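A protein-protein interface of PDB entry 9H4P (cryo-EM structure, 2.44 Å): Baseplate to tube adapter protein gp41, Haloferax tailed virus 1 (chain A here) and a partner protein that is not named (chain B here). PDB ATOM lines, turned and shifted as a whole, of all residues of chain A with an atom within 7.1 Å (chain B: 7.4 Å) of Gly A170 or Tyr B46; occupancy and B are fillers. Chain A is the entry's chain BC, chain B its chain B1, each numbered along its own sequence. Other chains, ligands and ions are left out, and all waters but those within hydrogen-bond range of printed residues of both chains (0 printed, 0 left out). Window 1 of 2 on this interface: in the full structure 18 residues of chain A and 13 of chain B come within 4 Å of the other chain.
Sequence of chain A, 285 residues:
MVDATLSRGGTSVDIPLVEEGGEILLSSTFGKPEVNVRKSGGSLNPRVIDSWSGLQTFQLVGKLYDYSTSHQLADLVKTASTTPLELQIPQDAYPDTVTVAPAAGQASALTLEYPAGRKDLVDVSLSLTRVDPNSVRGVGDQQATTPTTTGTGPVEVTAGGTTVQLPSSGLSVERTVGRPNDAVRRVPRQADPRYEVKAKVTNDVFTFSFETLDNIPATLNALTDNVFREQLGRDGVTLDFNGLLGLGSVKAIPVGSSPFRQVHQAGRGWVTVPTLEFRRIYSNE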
ATOM      1  N   PRO A 115      -9.031 -17.887 -10.828  1.00  0.00           N
ATOM      2  CA  PRO A 115      -8.676 -18.925  -9.855  1.00  0.00           C
ATOM      3  C   PRO A 115      -7.172 -19.193  -9.793  1.00  0.00           C
ATOM      4  O   PRO A 115      -6.433 -18.829 -10.711  1.00  0.00           O
ATOM      5  CB  PRO A 115      -9.443 -20.170 -10.344  1.00  0.00           C
ATOM      6  CG  PRO A 115      -9.628 -19.948 -11.834  1.00  0.00           C
ATOM      7  CD  PRO A 115      -9.761 -18.445 -11.985  1.00  0.00           C
ATOM      8  N   ALA A 116      -6.744 -19.834  -8.695  1.00  0.00           N
ATOM      9  CA  ALA A 116      -5.383 -20.327  -8.530  1.00  0.00           C
ATOM     10  C   ALA A 116      -5.050 -21.348  -9.624  1.00  0.00           C
ATOM     11  O   ALA A 116      -5.925 -22.105 -10.048  1.00  0.00           O
ATOM     12  CB  ALA A 116      -5.221 -20.922  -7.149  1.00  0.00           C
ATOM     13  N   GLY A 117      -3.776 -21.382 -10.051  1.00  0.00           N
ATOM     14  CA  GLY A 117      -3.368 -22.082 -11.263  1.00  0.00           C
ATOM     15  C   GLY A 117      -3.724 -21.230 -12.482  1.00  0.00           C
ATOM     16  O   GLY A 117      -3.496 -20.021 -12.444  1.00  0.00           O
ATOM     17  N   ARG A 118      -4.255 -21.864 -13.543  1.00  0.00           N
ATOM     18  CA  ARG A 118      -5.185 -21.255 -14.497  1.00  0.00           C
ATOM     19  C   ARG A 118      -4.690 -19.923 -15.085  1.00  0.00           C
ATOM     20  O   ARG A 118      -5.468 -18.967 -15.165  1.00  0.00           O
ATOM     21  CB  ARG A 118      -6.572 -21.083 -13.850  1.00  0.00           C
ATOM     22  CG  ARG A 118      -7.243 -22.372 -13.390  1.00  0.00           C
ATOM     23  CD  ARG A 118      -8.215 -22.957 -14.401  1.00  0.00           C
ATOM     24  NE  ARG A 118      -8.870 -24.133 -13.843  1.00  0.00           N
ATOM     25  CZ  ARG A 118     -10.126 -24.205 -13.406  1.00  0.00           C
ATOM     26  NH1 ARG A 118     -10.577 -25.345 -12.918  1.00  0.00           N
ATOM     27  NH2 ARG A 118     -10.932 -23.160 -13.472  1.00  0.00           N
ATOM     28  N   PRO A 167      -0.524 -12.970   0.757  1.00  0.00           N
ATOM     29  CA  PRO A 167       0.257 -14.116   0.281  1.00  0.00           C
ATOM     30  C   PRO A 167      -0.111 -14.505  -1.150  1.00  0.00           C
ATOM     31  O   PRO A 167      -1.277 -14.421  -1.544  1.00  0.00           O
ATOM     32  CB  PRO A 167      -0.137 -15.276   1.212  1.00  0.00           C
ATOM     33  CG  PRO A 167      -0.657 -14.596   2.456  1.00  0.00           C
ATOM     34  CD  PRO A 167      -1.274 -13.292   1.986  1.00  0.00           C
ATOM     35  N   SER A 168       0.906 -14.929  -1.913  1.00  0.00           N
ATOM     36  CA  SER A 168       0.725 -15.523  -3.230  1.00  0.00           C
ATOM     37  C   SER A 168       0.110 -16.924  -3.122  1.00  0.00           C
ATOM     38  O   SER A 168      -0.584 -17.365  -4.039  1.00  0.00           O
ATOM     39  CB  SER A 168       2.032 -15.559  -3.992  1.00  0.00           C
ATOM     40  OG  SER A 168       3.018 -16.289  -3.275  1.00  0.00           O
ATOM     41  N   SER A 169       0.389 -17.615  -2.004  1.00  0.00           N
ATOM     42  CA  SER A 169       0.064 -19.022  -1.790  1.00  0.00           C
ATOM     43  C   SER A 169      -1.447 -19.257  -1.723  1.00  0.00           C
ATOM     44  O   SER A 169      -2.114 -18.795  -0.793  1.00  0.00           O
ATOM     45  CB  SER A 169       0.767 -19.554  -0.561  1.00  0.00           C
ATOM     46  OG  SER A 169       0.451 -18.779   0.589  1.00  0.00           O
ATOM     47  N   GLY A 170      -1.968 -19.988  -2.723  1.00  0.00           N
ATOM     48  CA  GLY A 170      -3.382 -20.327  -2.829  1.00  0.00           C
ATOM     49  C   GLY A 170      -4.274 -19.145  -3.218  1.00  0.00           C
ATOM     50  O   GLY A 170      -5.496 -19.265  -3.131  1.00  0.00           O
ATOM     51  N   LEU A 171      -3.672 -18.024  -3.651  1.00  0.00           N
ATOM     52  CA  LEU A 171      -4.407 -16.798  -3.940  1.00  0.00           C
ATOM     53  C   LEU A 171      -5.397 -17.028  -5.090  1.00  0.00           C
ATOM     54  O   LEU A 171      -5.043 -17.629  -6.106  1.00  0.00           O
ATOM     55  CB  LEU A 171      -3.420 -15.660  -4.249  1.00  0.00           C
ATOM     56  CG  LEU A 171      -4.033 -14.270  -4.460  1.00  0.00           C
ATOM     57  CD1 LEU A 171      -4.666 -13.723  -3.181  1.00  0.00           C
ATOM     58  CD2 LEU A 171      -3.001 -13.286  -5.003  1.00  0.00           C
ATOM     59  N   SER A 172      -6.646 -16.572  -4.893  1.00  0.00           N
ATOM     60  CA  SER A 172      -7.679 -16.491  -5.921  1.00  0.00           C
ATOM     61  C   SER A 172      -8.374 -15.130  -5.832  1.00  0.00           C
ATOM     62  O   SER A 172      -8.595 -14.627  -4.728  1.00  0.00           O
ATOM     63  CB  SER A 172      -8.690 -17.601  -5.775  1.00  0.00           C
ATOM     64  OG  SER A 172      -8.075 -18.869  -5.929  1.00  0.00           O
ATOM     65  N   VAL A 173      -8.726 -14.548  -6.991  1.00  0.00           N
ATOM     66  CA  VAL A 173      -9.470 -13.290  -7.049  1.00  0.00           C
ATOM     67  C   VAL A 173     -10.829 -13.548  -7.707  1.00  0.00           C
ATOM     68  O   VAL A 173     -10.899 -14.163  -8.774  1.00  0.00           O
ATOM     69  CB  VAL A 173      -8.686 -12.166  -7.775  1.00  0.00           C
ATOM     70  CG1 VAL A 173      -9.480 -10.865  -7.913  1.00  0.00           C
ATOM     71  CG2 VAL A 173      -7.331 -11.884  -7.132  1.00  0.00           C
ATOM     72  N   SER A 209      -9.214 -14.983  -1.770  1.00  0.00           N
ATOM     73  CA  SER A 209      -9.069 -16.187  -0.967  1.00  0.00           C
ATOM     74  C   SER A 209      -7.597 -16.596  -1.018  1.00  0.00           C
ATOM     75  O   SER A 209      -7.004 -16.568  -2.096  1.00  0.00           O
ATOM     76  CB  SER A 209      -9.966 -17.280  -1.504  1.00  0.00           C
ATOM     77  OG  SER A 209     -10.005 -18.391  -0.620  1.00  0.00           O
ATOM     78  N   PHE A 210      -7.008 -16.962   0.133  1.00  0.00           N
ATOM     79  CA  PHE A 210      -5.579 -17.263   0.210  1.00  0.00           C
ATOM     80  C   PHE A 210      -5.257 -18.027   1.496  1.00  0.00           C
ATOM     81  O   PHE A 210      -6.093 -18.113   2.398  1.00  0.00           O
ATOM     82  CB  PHE A 210      -4.734 -15.982   0.117  1.00  0.00           C
ATOM     83  CG  PHE A 210      -5.075 -14.898   1.113  1.00  0.00           C
ATOM     84  CD1 PHE A 210      -4.508 -14.884   2.385  1.00  0.00           C
ATOM     85  CD2 PHE A 210      -5.962 -13.878   0.774  1.00  0.00           C
ATOM     86  CE1 PHE A 210      -4.822 -13.878   3.290  1.00  0.00           C
ATOM     87  CE2 PHE A 210      -6.282 -12.877   1.683  1.00  0.00           C
ATOM     88  CZ  PHE A 210      -5.710 -12.879   2.939  1.00  0.00           C
ATOM     89  N   GLU A 211      -4.025 -18.555   1.580  1.00  0.00           N
ATOM     90  CA  GLU A 211      -3.541 -19.217   2.784  1.00  0.00           C
ATOM     91  C   GLU A 211      -2.229 -18.559   3.226  1.00  0.00           C
ATOM     92  O   GLU A 211      -1.267 -18.535   2.457  1.00  0.00           O
ATOM     93  CB  GLU A 211      -3.446 -20.732   2.544  1.00  0.00           C
ATOM     94  CG  GLU A 211      -4.765 -21.336   2.071  1.00  0.00           C
ATOM     95  CD  GLU A 211      -4.848 -22.844   1.917  1.00  0.00           C
ATOM     96  OE1 GLU A 211      -4.250 -23.562   2.731  1.00  0.00           O
ATOM     97  OE2 GLU A 211      -5.509 -23.300   0.970  1.00  0.00           O
ATOM     98  N   LEU A 213       1.124 -18.619   5.058  1.00  0.00           N
ATOM     99  CA  LEU A 213       1.990 -19.755   5.360  1.00  0.00           C
ATOM    100  C   LEU A 213       3.175 -19.389   6.261  1.00  0.00           C
ATOM    101  O   LEU A 213       3.705 -20.266   6.946  1.00  0.00           O
ATOM    102  CB  LEU A 213       2.488 -20.386   4.052  1.00  0.00           C
ATOM    103  CG  LEU A 213       1.433 -20.940   3.087  1.00  0.00           C
ATOM    104  CD1 LEU A 213       2.105 -21.630   1.909  1.00  0.00           C
ATOM    105  CD2 LEU A 213       0.485 -21.917   3.772  1.00  0.00           C
ATOM    106  N   VAL A 273      -7.578 -18.234   4.804  1.00  0.00           N
ATOM    107  CA  VAL A 273      -8.518 -17.129   4.681  1.00  0.00           C
ATOM    108  C   VAL A 273      -9.508 -17.502   3.572  1.00  0.00           C
ATOM    109  O   VAL A 273      -9.165 -17.421   2.386  1.00  0.00           O
ATOM    110  CB  VAL A 273      -7.799 -15.777   4.448  1.00  0.00           C
ATOM    111  CG1 VAL A 273      -8.759 -14.643   4.085  1.00  0.00           C
ATOM    112  CG2 VAL A 273      -6.949 -15.376   5.653  1.00  0.00           C
ATOM    113  N   ALA B  43      -0.466 -30.279   1.026  1.00  0.00           N
ATOM    114  CA  ALA B  43      -1.229 -29.267   0.312  1.00  0.00           C
ATOM    115  C   ALA B  43      -0.319 -28.584  -0.712  1.00  0.00           C
ATOM    116  O   ALA B  43       0.624 -27.892  -0.325  1.00  0.00           O
ATOM    117  CB  ALA B  43      -1.827 -28.281   1.296  1.00  0.00           C
ATOM    118  N   GLU B  44      -0.594 -28.800  -2.011  1.00  0.00           N
ATOM    119  CA  GLU B  44       0.092 -28.108  -3.098  1.00  0.00           C
ATOM    120  C   GLU B  44      -0.728 -26.872  -3.479  1.00  0.00           C
ATOM    121  O   GLU B  44      -1.932 -26.983  -3.724  1.00  0.00           O
ATOM    122  CB  GLU B  44       0.270 -29.032  -4.308  1.00  0.00           C
ATOM    123  CG  GLU B  44       1.232 -30.183  -4.079  1.00  0.00           C
ATOM    124  CD  GLU B  44       1.518 -30.997  -5.327  1.00  0.00           C
ATOM    125  OE1 GLU B  44       0.573 -31.596  -5.869  1.00  0.00           O
ATOM    126  OE2 GLU B  44       2.682 -31.030  -5.751  1.00  0.00           O
ATOM    127  N   LEU B  45      -0.071 -25.700  -3.527  1.00  0.00           N
ATOM    128  CA  LEU B  45      -0.756 -24.414  -3.621  1.00  0.00           C
ATOM    129  C   LEU B  45      -0.252 -23.627  -4.834  1.00  0.00           C
ATOM    130  O   LEU B  45       0.935 -23.690  -5.160  1.00  0.00           O
ATOM    131  CB  LEU B  45      -0.551 -23.639  -2.309  1.00  0.00           C
ATOM    132  CG  LEU B  45      -1.146 -24.280  -1.048  1.00  0.00           C
ATOM    133  CD1 LEU B  45      -0.582 -23.642   0.215  1.00  0.00           C
ATOM    134  CD2 LEU B  45      -2.673 -24.215  -1.044  1.00  0.00           C
ATOM    135  N   TYR B  46      -1.163 -22.875  -5.482  1.00  0.00           N
ATOM    136  CA  TYR B  46      -0.915 -22.183  -6.745  1.00  0.00           C
ATOM    137  C   TYR B  46      -1.299 -20.699  -6.617  1.00  0.00           C
ATOM    138  O   TYR B  46      -2.119 -20.355  -5.763  1.00  0.00           O
ATOM    139  CB  TYR B  46      -1.673 -22.899  -7.876  1.00  0.00           C
ATOM    140  CG  TYR B  46      -1.213 -24.309  -8.180  1.00  0.00           C
ATOM    141  CD1 TYR B  46      -1.633 -25.399  -7.417  1.00  0.00           C
ATOM    142  CD2 TYR B  46      -0.351 -24.559  -9.242  1.00  0.00           C
ATOM    143  CE1 TYR B  46      -1.192 -26.689  -7.691  1.00  0.00           C
ATOM    144  CE2 TYR B  46       0.092 -25.844  -9.532  1.00  0.00           C
ATOM    145  CZ  TYR B  46      -0.326 -26.914  -8.752  1.00  0.00           C
ATOM    146  OH  TYR B  46       0.104 -28.178  -9.044  1.00  0.00           O
ATOM    147  N   THR B  47      -0.715 -19.823  -7.463  1.00  0.00           N
ATOM    148  CA  THR B  47      -1.054 -18.396  -7.518  1.00  0.00           C
ATOM    149  C   THR B  47      -2.087 -18.136  -8.626  1.00  0.00           C
ATOM    150  O   THR B  47      -2.443 -19.059  -9.361  1.00  0.00           O
ATOM    151  CB  THR B  47       0.180 -17.496  -7.735  1.00  0.00           C
ATOM    152  OG1 THR B  47       0.545 -17.474  -9.115  1.00  0.00           O
ATOM    153  CG2 THR B  47       1.397 -17.890  -6.931  1.00  0.00           C
ATOM    154  N   ILE B  48      -2.507 -16.866  -8.797  1.00  0.00           N
ATOM    155  CA  ILE B  48      -3.535 -16.457  -9.757  1.00  0.00           C
ATOM    156  C   ILE B  48      -3.049 -16.396 -11.213  1.00  0.00           C
ATOM    157  O   ILE B  48      -3.888 -16.321 -12.113  1.00  0.00           O
ATOM    158  CB  ILE B  48      -4.191 -15.107  -9.366  1.00  0.00           C
ATOM    159  CG1 ILE B  48      -3.175 -13.967  -9.187  1.00  0.00           C
ATOM    160  CG2 ILE B  48      -5.117 -15.262  -8.167  1.00  0.00           C
ATOM    161  CD1 ILE B  48      -3.783 -12.586  -8.988  1.00  0.00           C
ATOM    162  N   ASP B  49      -1.725 -16.394 -11.455  1.00  0.00           N
ATOM    163  CA  ASP B  49      -1.191 -16.013 -12.761  1.00  0.00           C
ATOM    164  C   ASP B  49      -0.090 -16.974 -13.225  1.00  0.00           C
ATOM    165  O   ASP B  49       0.794 -16.587 -13.993  1.00  0.00           O
ATOM    166  CB  ASP B  49      -0.749 -14.538 -12.763  1.00  0.00           C
ATOM    167  CG  ASP B  49      -0.543 -13.915 -14.138  1.00  0.00           C
ATOM    168  OD1 ASP B  49      -1.142 -14.407 -15.114  1.00  0.00           O
ATOM    169  OD2 ASP B  49       0.218 -12.931 -14.219  1.00  0.00           O
ATOM    170  N   SER B  50      -0.163 -18.234 -12.775  1.00  0.00           N
ATOM    171  CA  SER B  50       0.832 -19.240 -13.115  1.00  0.00           C
ATOM    172  C   SER B  50       0.211 -20.634 -13.039  1.00  0.00           C
ATOM    173  O   SER B  50      -0.583 -20.915 -12.142  1.00  0.00           O
ATOM    174  CB  SER B  50       2.045 -19.124 -12.206  1.00  0.00           C
ATOM    175  OG  SER B  50       2.991 -20.156 -12.454  1.00  0.00           O
ATOM    176  N   THR B  51       0.624 -21.499 -13.975  1.00  0.00           N
ATOM    177  CA  THR B  51       0.320 -22.925 -13.948  1.00  0.00           C
ATOM    178  C   THR B  51       1.199 -23.661 -12.933  1.00  0.00           C
ATOM    179  O   THR B  51       0.866 -24.778 -12.535  1.00  0.00           O
ATOM    180  CB  THR B  51       0.508 -23.576 -15.329  1.00  0.00           C
ATOM    181  OG1 THR B  51       1.869 -23.463 -15.753  1.00  0.00           O
ATOM    182  CG2 THR B  51      -0.408 -23.009 -16.395  1.00  0.00           C
ATOM    183  N   PHE B  52       2.321 -23.047 -12.522  1.00  0.00           N
ATOM    184  CA  PHE B  52       3.295 -23.719 -11.667  1.00  0.00           C
ATOM    185  C   PHE B  52       2.922 -23.575 -10.189  1.00  0.00           C
ATOM    186  O   PHE B  52       2.346 -22.564  -9.779  1.00  0.00           O
ATOM    187  CB  PHE B  52       4.712 -23.189 -11.918  1.00  0.00           C
ATOM    188  CG  PHE B  52       5.370 -23.528 -13.237  1.00  0.00           C
ATOM    189  CD1 PHE B  52       4.751 -24.317 -14.208  1.00  0.00           C
ATOM    190  CD2 PHE B  52       6.659 -23.069 -13.486  1.00  0.00           C
ATOM    191  CE1 PHE B  52       5.402 -24.612 -15.400  1.00  0.00           C
ATOM    192  CE2 PHE B  52       7.312 -23.371 -14.674  1.00  0.00           C
ATOM    193  CZ  PHE B  52       6.681 -24.140 -15.631  1.00  0.00           C
ATOM    194  N   ARG B  53       3.275 -24.609  -9.411  1.00  0.00           N
ATOM    195  CA  ARG B  53       3.083 -24.683  -7.969  1.00  0.00           C
ATOM    196  C   ARG B  53       3.884 -23.575  -7.275  1.00  0.00           C
ATOM    197  O   ARG B  53       5.070 -23.392  -7.560  1.00  0.00           O
ATOM    198  CB  ARG B  53       3.514 -26.083  -7.512  1.00  0.00           C
ATOM    199  CG  ARG B  53       3.084 -26.476  -6.104  1.00  0.00           C
ATOM    200  CD  ARG B  53       3.575 -27.881  -5.794  1.00  0.00           C
ATOM    201  NE  ARG B  53       5.024 -27.941  -5.593  1.00  0.00           N
ATOM    202  CZ  ARG B  53       5.795 -29.034  -5.639  1.00  0.00           C
ATOM    203  NH1 ARG B  53       7.098 -28.920  -5.429  1.00  0.00           N
ATOM    204  NH2 ARG B  53       5.280 -30.228  -5.888  1.00  0.00           N
ATOM    205  N   ASP B  54       3.225 -22.854  -6.355  1.00  0.00           N
ATOM    206  CA  ASP B  54       3.832 -21.752  -5.618  1.00  0.00           C
ATOM    207  C   ASP B  54       4.555 -22.284  -4.380  1.00  0.00           C
ATOM    208  O   ASP B  54       5.734 -21.990  -4.166  1.00  0.00           O
ATOM    209  CB  ASP B  54       2.784 -20.699  -5.242  1.00  0.00           C
ATOM    210  CG  ASP B  54       3.372 -19.434  -4.637  1.00  0.00           C
ATOM    211  OD1 ASP B  54       4.499 -19.061  -5.020  1.00  0.00           O
ATOM    212  OD2 ASP B  54       2.689 -18.823  -3.798  1.00  0.00           O
ATOM    213  N   GLU B  55       3.817 -23.060  -3.572  1.00  0.00           N
ATOM    214  CA  GLU B  55       4.333 -23.677  -2.360  1.00  0.00           C
ATOM    215  C   GLU B  55       3.686 -25.045  -2.152  1.00  0.00           C
ATOM    216  O   GLU B  55       2.648 -25.352  -2.746  1.00  0.00           O
ATOM    217  CB  GLU B  55       4.111 -22.783  -1.133  1.00  0.00           C
ATOM    218  CG  GLU B  55       5.306 -21.913  -0.768  1.00  0.00           C
ATOM    219  CD  GLU B  55       6.641 -22.598  -0.515  1.00  0.00           C
ATOM    220  OE1 GLU B  55       6.699 -23.841  -0.493  1.00  0.00           O
ATOM    221  OE2 GLU B  55       7.630 -21.877  -0.328  1.00  0.00           O
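The backbone NH (N) of Gly A117 is in hydrogen-bond range of the backbone carbonyl oxygen (O) of Thr B47, 2.8 Å away. OG of Ser A168 sits at hydrogen-bond distance from OD2 of Asp B54 (2.6 Å). The side-chain carboxylate (OD2) of Asp B54 sits at hydrogen-bond distance from the backbone NH (N) of Ser A169 (3.2 Å). N of Gly A170 lies within hydrogen-bond range of O of Tyr B46. The backbone carbonyl oxygen (O) of Ser B50 sits close to the backbone carbonyl oxygen (O) of Gly A117.
The backbone NH of Ala A116 sits at hydrogen-bond distance from the side-chain hydroxyl of Ser A172, 3.2 Å away. The side-chain hydroxyl (OG) of Ser A169 is in hydrogen-bond range of the backbone carbonyl oxygen (O) of Glu A211. The backbone NH (N) of Ser A172 is in hydrogen-bond range of the backbone carbonyl oxygen (O) of Ser A209, at 2.8 Å. The backbone carbonyl oxygen of Glu B55 sits at hydrogen-bond distance from the backbone NH of Leu B45 (2.9 Å). OG1 of Thr B47 lies close to N of Asp B49. The side-chain hydroxyl of Ser B50 sits at hydrogen-bond distance from the backbone NH of Phe B52, at 3.0 Å.
Among the printed residues, merely in contact across the chains: Leu A171 with Ile B48, Ala A116 with Thr B47, Gly A117 with Tyr B46, Ala A116 with Tyr B46, Leu A171 with Tyr B46, Ser A168 with Thr B47, Glu A211 with Leu B45, Ser A172 with Ile B48, Gly A117 with Ile B48, Leu A213 with Leu B45, Ser A168 with Tyr B46, Leu A213 with Glu B55, Pro A115 with Ile B48, Val A173 with Ile B48, Leu A171 with Thr B47 and Gly A170 with Leu B45.
Gly A170 touches just these residues of chain B: Leu B45 (3.9 Å) and Tyr B46 (3.1 Å). Tyr B46 touches five residues of chain A. Printed residues of chain A within 4 Å of Glu B55: Leu A213. Printed residues of chain A within 4 Å of Asp B54: Ser A168 (2.6 Å) and Ser A169 (3.2 Å). Of the printed residues of chain A, Ser B50 touches Gly A117 (3.1 Å). Printed residues of chain A within 4 Å of Leu B45: Gly A170 (3.9 Å), Glu A211 (3.6 Å) and Leu A213 (3.8 Å). The nearest printed residue of chain B that does not touch Gly A170 is Thr B47 (4.9 Å). The nearest printed residue of chain B that does not touch Leu A213 is Asp B54 (6.4 Å).
Printed residues of chain B that touch a printed residue of chain A: Leu B45, Tyr B46, Thr B47, Ile B48, Ser B50, Asp B54 and Glu B55. Hydrophobic or aromatic side chains of chain B that line the printed part of chain A: Leu B45, Tyr B46 and Ile B48. Along chain B the printed residues that touch a printed residue of chain A span positions 45 to 55. Hydrophobic or aromatic side chains of chain A within 4 Å of the printed part of chain B: Ala A116, Leu A171 and Leu A213. Along chain A the printed residues that touch a printed residue of chain B span positions 115 to 213. Among the printed residues, 21 pairs touch across the chains. Among the printed residues, no Asp or Glu carboxylate lies within 4 Å of a Lys or Arg side-chain nitrogen of the other chain.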
